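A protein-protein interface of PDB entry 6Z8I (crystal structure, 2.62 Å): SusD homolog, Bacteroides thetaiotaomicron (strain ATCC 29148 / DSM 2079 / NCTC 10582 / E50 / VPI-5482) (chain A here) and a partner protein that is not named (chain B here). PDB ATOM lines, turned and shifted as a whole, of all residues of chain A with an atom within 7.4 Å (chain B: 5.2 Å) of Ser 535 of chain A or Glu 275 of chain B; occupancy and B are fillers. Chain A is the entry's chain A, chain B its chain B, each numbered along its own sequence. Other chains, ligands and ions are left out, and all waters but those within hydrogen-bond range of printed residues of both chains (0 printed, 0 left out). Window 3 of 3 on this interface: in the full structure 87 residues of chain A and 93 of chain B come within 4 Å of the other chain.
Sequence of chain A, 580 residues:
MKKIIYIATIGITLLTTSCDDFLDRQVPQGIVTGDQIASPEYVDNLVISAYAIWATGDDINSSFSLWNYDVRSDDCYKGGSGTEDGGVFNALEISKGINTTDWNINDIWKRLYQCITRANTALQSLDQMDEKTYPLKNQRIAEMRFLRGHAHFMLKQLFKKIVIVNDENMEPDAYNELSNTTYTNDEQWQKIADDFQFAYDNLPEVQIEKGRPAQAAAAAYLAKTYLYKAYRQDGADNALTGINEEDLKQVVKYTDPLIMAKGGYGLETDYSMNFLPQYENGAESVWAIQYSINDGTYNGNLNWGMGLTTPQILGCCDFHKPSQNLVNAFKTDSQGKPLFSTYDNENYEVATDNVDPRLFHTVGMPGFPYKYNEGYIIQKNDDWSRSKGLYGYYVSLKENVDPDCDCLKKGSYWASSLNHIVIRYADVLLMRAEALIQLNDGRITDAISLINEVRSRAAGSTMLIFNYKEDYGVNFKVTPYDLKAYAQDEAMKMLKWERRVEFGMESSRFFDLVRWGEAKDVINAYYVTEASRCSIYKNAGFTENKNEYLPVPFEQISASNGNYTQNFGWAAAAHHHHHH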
ATOM      1  N   THR A  83      14.133  12.019 -22.973  1.00  0.00           N
ATOM      2  CA  THR A  83      14.659  12.063 -21.612  1.00  0.00           C
ATOM      3  C   THR A  83      15.874  12.966 -21.501  1.00  0.00           C
ATOM      4  O   THR A  83      16.097  13.580 -20.449  1.00  0.00           O
ATOM      5  CB  THR A  83      15.040  10.665 -21.143  1.00  0.00           C
ATOM      6  OG1 THR A  83      14.120   9.715 -21.677  1.00  0.00           O
ATOM      7  CG2 THR A  83      14.998  10.587 -19.637  1.00  0.00           C
ATOM      8  N   GLU A  84      16.669  13.054 -22.565  1.00  0.00           N
ATOM      9  CA  GLU A  84      17.943  13.753 -22.515  1.00  0.00           C
ATOM     10  C   GLU A  84      17.784  15.259 -22.512  1.00  0.00           C
ATOM     11  O   GLU A  84      18.777  15.959 -22.322  1.00  0.00           O
ATOM     12  CB  GLU A  84      18.822  13.308 -23.680  1.00  0.00           C
ATOM     13  CG  GLU A  84      19.046  11.798 -23.745  1.00  0.00           C
ATOM     14  CD  GLU A  84      17.923  11.051 -24.451  1.00  0.00           C
ATOM     15  OE1 GLU A  84      16.770  11.532 -24.431  1.00  0.00           O
ATOM     16  OE2 GLU A  84      18.196   9.985 -25.042  1.00  0.00           O
ATOM     17  N   ILE A  94      10.606  11.940 -11.866  1.00  0.00           N
ATOM     18  CA  ILE A  94      10.546  10.580 -11.346  1.00  0.00           C
ATOM     19  C   ILE A  94      11.096  10.478  -9.925  1.00  0.00           C
ATOM     20  O   ILE A  94      11.141   9.379  -9.363  1.00  0.00           O
ATOM     21  CB  ILE A  94      11.258   9.588 -12.283  1.00  0.00           C
ATOM     22  CG1 ILE A  94      12.777   9.797 -12.229  1.00  0.00           C
ATOM     23  CG2 ILE A  94      10.696   9.704 -13.680  1.00  0.00           C
ATOM     24  CD1 ILE A  94      13.560   8.764 -13.015  1.00  0.00           C
ATOM     25  N   GLY A 389       5.690  10.307 -29.636  1.00  0.00           N
ATOM     26  CA  GLY A 389       4.845   9.480 -28.809  1.00  0.00           C
ATOM     27  C   GLY A 389       5.356   9.241 -27.400  1.00  0.00           C
ATOM     28  O   GLY A 389       4.562   8.848 -26.531  1.00  0.00           O
ATOM     29  N   LEU A 390       6.652   9.455 -27.142  1.00  0.00           N
ATOM     30  CA  LEU A 390       7.197   9.113 -25.829  1.00  0.00           C
ATOM     31  C   LEU A 390       6.401   9.785 -24.718  1.00  0.00           C
ATOM     32  O   LEU A 390       5.880   9.111 -23.823  1.00  0.00           O
ATOM     33  CB  LEU A 390       8.682   9.482 -25.738  1.00  0.00           C
ATOM     34  CG  LEU A 390       9.503   8.963 -24.535  1.00  0.00           C
ATOM     35  CD1 LEU A 390       9.482   9.926 -23.366  1.00  0.00           C
ATOM     36  CD2 LEU A 390       9.038   7.566 -24.068  1.00  0.00           C
ATOM     37  N   TYR A 391       6.271  11.114 -24.776  1.00  0.00           N
ATOM     38  CA  TYR A 391       5.475  11.860 -23.808  1.00  0.00           C
ATOM     39  C   TYR A 391       4.022  12.058 -24.263  1.00  0.00           C
ATOM     40  O   TYR A 391       3.400  13.068 -23.911  1.00  0.00           O
ATOM     41  CB  TYR A 391       6.128  13.214 -23.514  1.00  0.00           C
ATOM     42  CG  TYR A 391       7.487  13.163 -22.821  1.00  0.00           C
ATOM     43  CD1 TYR A 391       7.585  12.962 -21.453  1.00  0.00           C
ATOM     44  CD2 TYR A 391       8.676  13.365 -23.538  1.00  0.00           C
ATOM     45  CE1 TYR A 391       8.825  12.934 -20.817  1.00  0.00           C
ATOM     46  CE2 TYR A 391       9.925  13.329 -22.910  1.00  0.00           C
ATOM     47  CZ  TYR A 391       9.992  13.116 -21.547  1.00  0.00           C
ATOM     48  OH  TYR A 391      11.213  13.086 -20.901  1.00  0.00           O
ATOM     49  N   GLU A 530       0.792   5.292 -14.093  1.00  0.00           N
ATOM     50  CA  GLU A 530       1.161   5.955 -15.338  1.00  0.00           C
ATOM     51  C   GLU A 530       2.196   5.179 -16.136  1.00  0.00           C
ATOM     52  O   GLU A 530       2.277   5.358 -17.353  1.00  0.00           O
ATOM     53  CB  GLU A 530       1.703   7.353 -15.034  1.00  0.00           C
ATOM     54  CG  GLU A 530       1.452   8.364 -16.124  1.00  0.00           C
ATOM     55  CD  GLU A 530       0.015   8.374 -16.598  1.00  0.00           C
ATOM     56  OE1 GLU A 530      -0.858   8.876 -15.868  1.00  0.00           O
ATOM     57  OE2 GLU A 530      -0.244   7.878 -17.708  1.00  0.00           O
ATOM     58  N   ALA A 531       2.989   4.327 -15.480  1.00  0.00           N
ATOM     59  CA  ALA A 531       4.126   3.700 -16.148  1.00  0.00           C
ATOM     60  C   ALA A 531       3.687   2.848 -17.327  1.00  0.00           C
ATOM     61  O   ALA A 531       4.437   2.708 -18.297  1.00  0.00           O
ATOM     62  CB  ALA A 531       4.927   2.858 -15.155  1.00  0.00           C
ATOM     63  N   SER A 532       2.482   2.272 -17.266  1.00  0.00           N
ATOM     64  CA  SER A 532       1.985   1.467 -18.382  1.00  0.00           C
ATOM     65  C   SER A 532       1.749   2.312 -19.638  1.00  0.00           C
ATOM     66  O   SER A 532       1.854   1.799 -20.760  1.00  0.00           O
ATOM     67  CB  SER A 532       0.703   0.734 -17.974  1.00  0.00           C
ATOM     68  OG  SER A 532      -0.124   1.540 -17.142  1.00  0.00           O
ATOM     69  N   ARG A 533       1.457   3.606 -19.477  1.00  0.00           N
ATOM     70  CA  ARG A 533       1.196   4.491 -20.605  1.00  0.00           C
ATOM     71  C   ARG A 533       2.394   5.341 -21.011  1.00  0.00           C
ATOM     72  O   ARG A 533       2.437   5.808 -22.153  1.00  0.00           O
ATOM     73  CB  ARG A 533       0.022   5.431 -20.289  1.00  0.00           C
ATOM     74  CG  ARG A 533      -1.280   4.722 -19.926  1.00  0.00           C
ATOM     75  CD  ARG A 533      -2.009   5.450 -18.797  1.00  0.00           C
ATOM     76  NE  ARG A 533      -3.356   4.929 -18.550  1.00  0.00           N
ATOM     77  CZ  ARG A 533      -4.187   5.429 -17.640  1.00  0.00           C
ATOM     78  NH1 ARG A 533      -3.812   6.466 -16.894  1.00  0.00           N
ATOM     79  NH2 ARG A 533      -5.391   4.902 -17.477  1.00  0.00           N
ATOM     80  N   CYS A 534       3.355   5.557 -20.113  1.00  0.00           N
ATOM     81  CA  CYS A 534       4.494   6.440 -20.354  1.00  0.00           C
ATOM     82  C   CYS A 534       5.712   5.846 -19.667  1.00  0.00           C
ATOM     83  O   CYS A 534       5.698   5.684 -18.444  1.00  0.00           O
ATOM     84  CB  CYS A 534       4.217   7.842 -19.819  1.00  0.00           C
ATOM     85  SG  CYS A 534       5.609   8.931 -19.982  1.00  0.00           S
ATOM     86  N   SER A 535       6.766   5.538 -20.442  1.00  0.00           N
ATOM     87  CA  SER A 535       7.834   4.656 -19.969  1.00  0.00           C
ATOM     88  C   SER A 535       8.869   5.354 -19.099  1.00  0.00           C
ATOM     89  O   SER A 535       9.688   4.664 -18.487  1.00  0.00           O
ATOM     90  CB  SER A 535       8.560   3.976 -21.138  1.00  0.00           C
ATOM     91  OG  SER A 535       8.928   4.896 -22.149  1.00  0.00           O
ATOM     92  N   ILE A 536       8.854   6.684 -19.023  1.00  0.00           N
ATOM     93  CA  ILE A 536       9.813   7.380 -18.174  1.00  0.00           C
ATOM     94  C   ILE A 536       9.609   7.035 -16.699  1.00  0.00           C
ATOM     95  O   ILE A 536      10.548   7.130 -15.895  1.00  0.00           O
ATOM     96  CB  ILE A 536       9.704   8.893 -18.399  1.00  0.00           C
ATOM     97  CG1 ILE A 536       8.343   9.356 -17.911  1.00  0.00           C
ATOM     98  CG2 ILE A 536       9.892   9.227 -19.866  1.00  0.00           C
ATOM     99  CD1 ILE A 536       8.394  10.641 -17.201  1.00  0.00           C
ATOM    100  N   TYR A 537       8.389   6.649 -16.316  1.00  0.00           N
ATOM    101  CA  TYR A 537       8.071   6.343 -14.925  1.00  0.00           C
ATOM    102  C   TYR A 537       8.422   4.908 -14.534  1.00  0.00           C
ATOM    103  O   TYR A 537       8.297   4.560 -13.356  1.00  0.00           O
ATOM    104  CB  TYR A 537       6.585   6.626 -14.647  1.00  0.00           C
ATOM    105  CG  TYR A 537       6.240   8.101 -14.677  1.00  0.00           C
ATOM    106  CD1 TYR A 537       6.672   8.964 -13.673  1.00  0.00           C
ATOM    107  CD2 TYR A 537       5.483   8.640 -15.719  1.00  0.00           C
ATOM    108  CE1 TYR A 537       6.350  10.337 -13.705  1.00  0.00           C
ATOM    109  CE2 TYR A 537       5.157  10.006 -15.760  1.00  0.00           C
ATOM    110  CZ  TYR A 537       5.592  10.845 -14.759  1.00  0.00           C
ATOM    111  OH  TYR A 537       5.267  12.182 -14.812  1.00  0.00           O
ATOM    112  N   LYS A 538       8.896   4.091 -15.482  1.00  0.00           N
ATOM    113  CA  LYS A 538       9.136   2.675 -15.222  1.00  0.00           C
ATOM    114  C   LYS A 538      10.073   2.457 -14.046  1.00  0.00           C
ATOM    115  O   LYS A 538       9.974   1.439 -13.361  1.00  0.00           O
ATOM    116  CB  LYS A 538       9.695   1.996 -16.478  1.00  0.00           C
ATOM    117  CG  LYS A 538      10.725   0.888 -16.223  1.00  0.00           C
ATOM    118  CD  LYS A 538      11.475   0.508 -17.505  1.00  0.00           C
ATOM    119  CE  LYS A 538      12.712  -0.349 -17.223  1.00  0.00           C
ATOM    120  NZ  LYS A 538      12.877  -1.459 -18.210  1.00  0.00           N
ATOM    121  N   ASN A 539      10.979   3.390 -13.782  1.00  0.00           N
ATOM    122  CA  ASN A 539      11.884   3.254 -12.646  1.00  0.00           C
ATOM    123  C   ASN A 539      11.678   4.365 -11.624  1.00  0.00           C
ATOM    124  O   ASN A 539      12.597   4.673 -10.866  1.00  0.00           O
ATOM    125  CB  ASN A 539      13.343   3.242 -13.112  1.00  0.00           C
ATOM    126  CG  ASN A 539      13.696   2.009 -13.927  1.00  0.00           C
ATOM    127  OD1 ASN A 539      13.269   0.892 -13.620  1.00  0.00           O
ATOM    128  ND2 ASN A 539      14.490   2.210 -14.979  1.00  0.00           N
ATOM    129  N   ALA A 540      10.506   4.996 -11.603  1.00  0.00           N
ATOM    130  CA  ALA A 540      10.297   6.130 -10.720  1.00  0.00           C
ATOM    131  C   ALA A 540      10.159   5.667  -9.270  1.00  0.00           C
ATOM    132  O   ALA A 540       9.983   4.480  -8.983  1.00  0.00           O
ATOM    133  CB  ALA A 540       9.064   6.908 -11.154  1.00  0.00           C
ATOM    134  N   TYR B 270      19.694   2.913 -25.695  1.00  0.00           N
ATOM    135  CA  TYR B 270      18.326   2.453 -25.506  1.00  0.00           C
ATOM    136  C   TYR B 270      18.308   1.069 -24.869  1.00  0.00           C
ATOM    137  O   TYR B 270      17.757   0.883 -23.781  1.00  0.00           O
ATOM    138  CB  TYR B 270      17.566   2.466 -26.835  1.00  0.00           C
ATOM    139  CG  TYR B 270      16.628   3.651 -26.992  1.00  0.00           C
ATOM    140  CD1 TYR B 270      15.269   3.519 -26.764  1.00  0.00           C
ATOM    141  CD2 TYR B 270      17.110   4.899 -27.365  1.00  0.00           C
ATOM    142  CE1 TYR B 270      14.411   4.599 -26.907  1.00  0.00           C
ATOM    143  CE2 TYR B 270      16.268   5.984 -27.508  1.00  0.00           C
ATOM    144  CZ  TYR B 270      14.918   5.831 -27.275  1.00  0.00           C
ATOM    145  OH  TYR B 270      14.064   6.900 -27.414  1.00  0.00           O
ATOM    146  N   VAL B 271      18.940   0.085 -25.515  1.00  0.00           N
ATOM    147  CA  VAL B 271      18.882  -1.280 -24.994  1.00  0.00           C
ATOM    148  C   VAL B 271      19.558  -1.376 -23.633  1.00  0.00           C
ATOM    149  O   VAL B 271      19.202  -2.231 -22.818  1.00  0.00           O
ATOM    150  CB  VAL B 271      19.490  -2.271 -26.003  1.00  0.00           C
ATOM    151  CG1 VAL B 271      18.475  -2.579 -27.085  1.00  0.00           C
ATOM    152  CG2 VAL B 271      20.767  -1.709 -26.603  1.00  0.00           C
ATOM    153  N   ASP B 273      19.083   0.563 -21.316  1.00  0.00           N
ATOM    154  CA  ASP B 273      18.036   0.957 -20.384  1.00  0.00           C
ATOM    155  C   ASP B 273      16.792   0.081 -20.486  1.00  0.00           C
ATOM    156  O   ASP B 273      15.764   0.412 -19.887  1.00  0.00           O
ATOM    157  CB  ASP B 273      17.651   2.422 -20.608  1.00  0.00           C
ATOM    158  CG  ASP B 273      18.672   3.400 -20.048  1.00  0.00           C
ATOM    159  OD1 ASP B 273      18.519   4.617 -20.319  1.00  0.00           O
ATOM    160  OD2 ASP B 273      19.620   2.966 -19.344  1.00  0.00           O
ATOM    161  N   GLY B 274      16.857  -1.023 -21.230  1.00  0.00           N
ATOM    162  CA  GLY B 274      15.691  -1.864 -21.435  1.00  0.00           C
ATOM    163  C   GLY B 274      14.523  -1.082 -21.990  1.00  0.00           C
ATOM    164  O   GLY B 274      13.442  -1.068 -21.397  1.00  0.00           O
ATOM    165  N   GLU B 275      14.748  -0.398 -23.111  1.00  0.00           N
ATOM    166  CA  GLU B 275      13.740   0.393 -23.797  1.00  0.00           C
ATOM    167  C   GLU B 275      13.717  -0.005 -25.264  1.00  0.00           C
ATOM    168  O   GLU B 275      14.743  -0.385 -25.831  1.00  0.00           O
ATOM    169  CB  GLU B 275      14.024   1.891 -23.681  1.00  0.00           C
ATOM    170  CG  GLU B 275      13.486   2.569 -22.431  1.00  0.00           C
ATOM    171  CD  GLU B 275      13.402   4.090 -22.593  1.00  0.00           C
ATOM    172  OE1 GLU B 275      12.651   4.554 -23.480  1.00  0.00           O
ATOM    173  OE2 GLU B 275      14.093   4.824 -21.846  1.00  0.00           O
ATOM    174  N   ASN B 276      12.546   0.090 -25.883  1.00  0.00           N
ATOM    175  CA  ASN B 276      12.434  -0.262 -27.296  1.00  0.00           C
ATOM    176  C   ASN B 276      13.190   0.744 -28.146  1.00  0.00           C
ATOM    177  O   ASN B 276      12.688   1.858 -28.354  1.00  0.00           O
ATOM    178  CB  ASN B 276      10.975  -0.316 -27.740  1.00  0.00           C
ATOM    179  CG  ASN B 276      10.789  -1.106 -29.022  1.00  0.00           C
ATOM    180  OD1 ASN B 276      11.744  -1.335 -29.770  1.00  0.00           O
ATOM    181  ND2 ASN B 276       9.557  -1.535 -29.279  1.00  0.00           N
ATOM    182  N   PRO B 277      14.365   0.397 -28.678  1.00  0.00           N
ATOM    183  CA  PRO B 277      15.137   1.379 -29.450  1.00  0.00           C
ATOM    184  C   PRO B 277      14.438   1.821 -30.728  1.00  0.00           C
ATOM    185  O   PRO B 277      14.764   2.891 -31.260  1.00  0.00           O
ATOM    186  CB  PRO B 277      16.446   0.640 -29.738  1.00  0.00           C
ATOM    187  CG  PRO B 277      16.033  -0.823 -29.798  1.00  0.00           C
ATOM    188  CD  PRO B 277      14.856  -0.983 -28.874  1.00  0.00           C
ATOM    189  N   ARG B 954      20.362   7.072 -21.362  1.00  0.00           N
ATOM    190  CA  ARG B 954      19.601   8.275 -21.685  1.00  0.00           C
ATOM    191  C   ARG B 954      19.380   9.173 -20.481  1.00  0.00           C
ATOM    192  O   ARG B 954      18.709  10.202 -20.613  1.00  0.00           O
ATOM    193  CB  ARG B 954      18.233   7.918 -22.287  1.00  0.00           C
ATOM    194  CG  ARG B 954      18.257   6.805 -23.314  1.00  0.00           C
ATOM    195  CD  ARG B 954      17.292   7.095 -24.450  1.00  0.00           C
ATOM    196  NE  ARG B 954      15.917   7.280 -23.994  1.00  0.00           N
ATOM    197  CZ  ARG B 954      15.014   7.999 -24.649  1.00  0.00           C
ATOM    198  NH1 ARG B 954      13.785   8.122 -24.172  1.00  0.00           N
ATOM    199  NH2 ARG B 954      15.346   8.604 -25.779  1.00  0.00           N
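The guanidinium group (NH2) of Arg 954 of chain B is in salt-bridge range of the side-chain carboxylate (OE2) of Glu 84 of chain A (3.3 Å). The side-chain hydroxyl (OG1) of Thr 83 of chain A is in hydrogen-bond range of the guanidinium group (NH1) of Arg 954 of chain B (3.0 Å). O of Gly 274 of chain B lies within hydrogen-bond range of NZ of Lys 538 of chain A.
OH of Tyr 270 of chain B sits at hydrogen-bond distance from NH2 of Arg 954 of chain B (2.7 Å). OD1 of Asp 273 of chain B is in hydrogen-bond range of N of Arg 954 of chain B, at 3.2 Å. The side-chain carboxylate (OE2) of Glu 275 of chain B lies within salt-bridge range of the guanidinium group (NE) of Arg 954 of chain B, 3.7 Å away. The backbone carbonyl oxygen (O) of Tyr 270 of chain B lies within hydrogen-bond range of the backbone NH (N) of Glu 275 of chain B (3.3 Å).
Among the printed residues, merely in contact across the chains: Ser 535 of chain A with Glu 275 of chain B (3.97 Å) and Lys 538 of chain A with Asp 273 of chain B (3.8 Å).
Of the printed residues of chain B, Thr 83 of chain A touches Arg 954. Of chain B, only Glu 275 (3.97 Å) comes within 4 Å of Ser 535 of chain A. Of the printed residues of chain B, Lys 538 of chain A touches Asp 273 and Gly 274. Of the printed residues of chain A, Asp 273 of chain B touches Lys 538. Of the printed residues of chain A, Gly 274 of chain B touches Lys 538 (3.3 Å). Of chain A, only Ser 535 comes within 4 Å of Glu 275 of chain B. The nearest printed residue of chain B that does not touch Lys 538 of chain A is Glu 275 of chain B (5.4 Å).
Of the 17 printed residues of chain A, 4 touch a printed residue of chain B. Printed residues of chain A that touch a printed residue of chain B: Thr 83, Glu 84, Ser 535 and Lys 538. Among the printed residues, 5 pairs touch across the chains.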
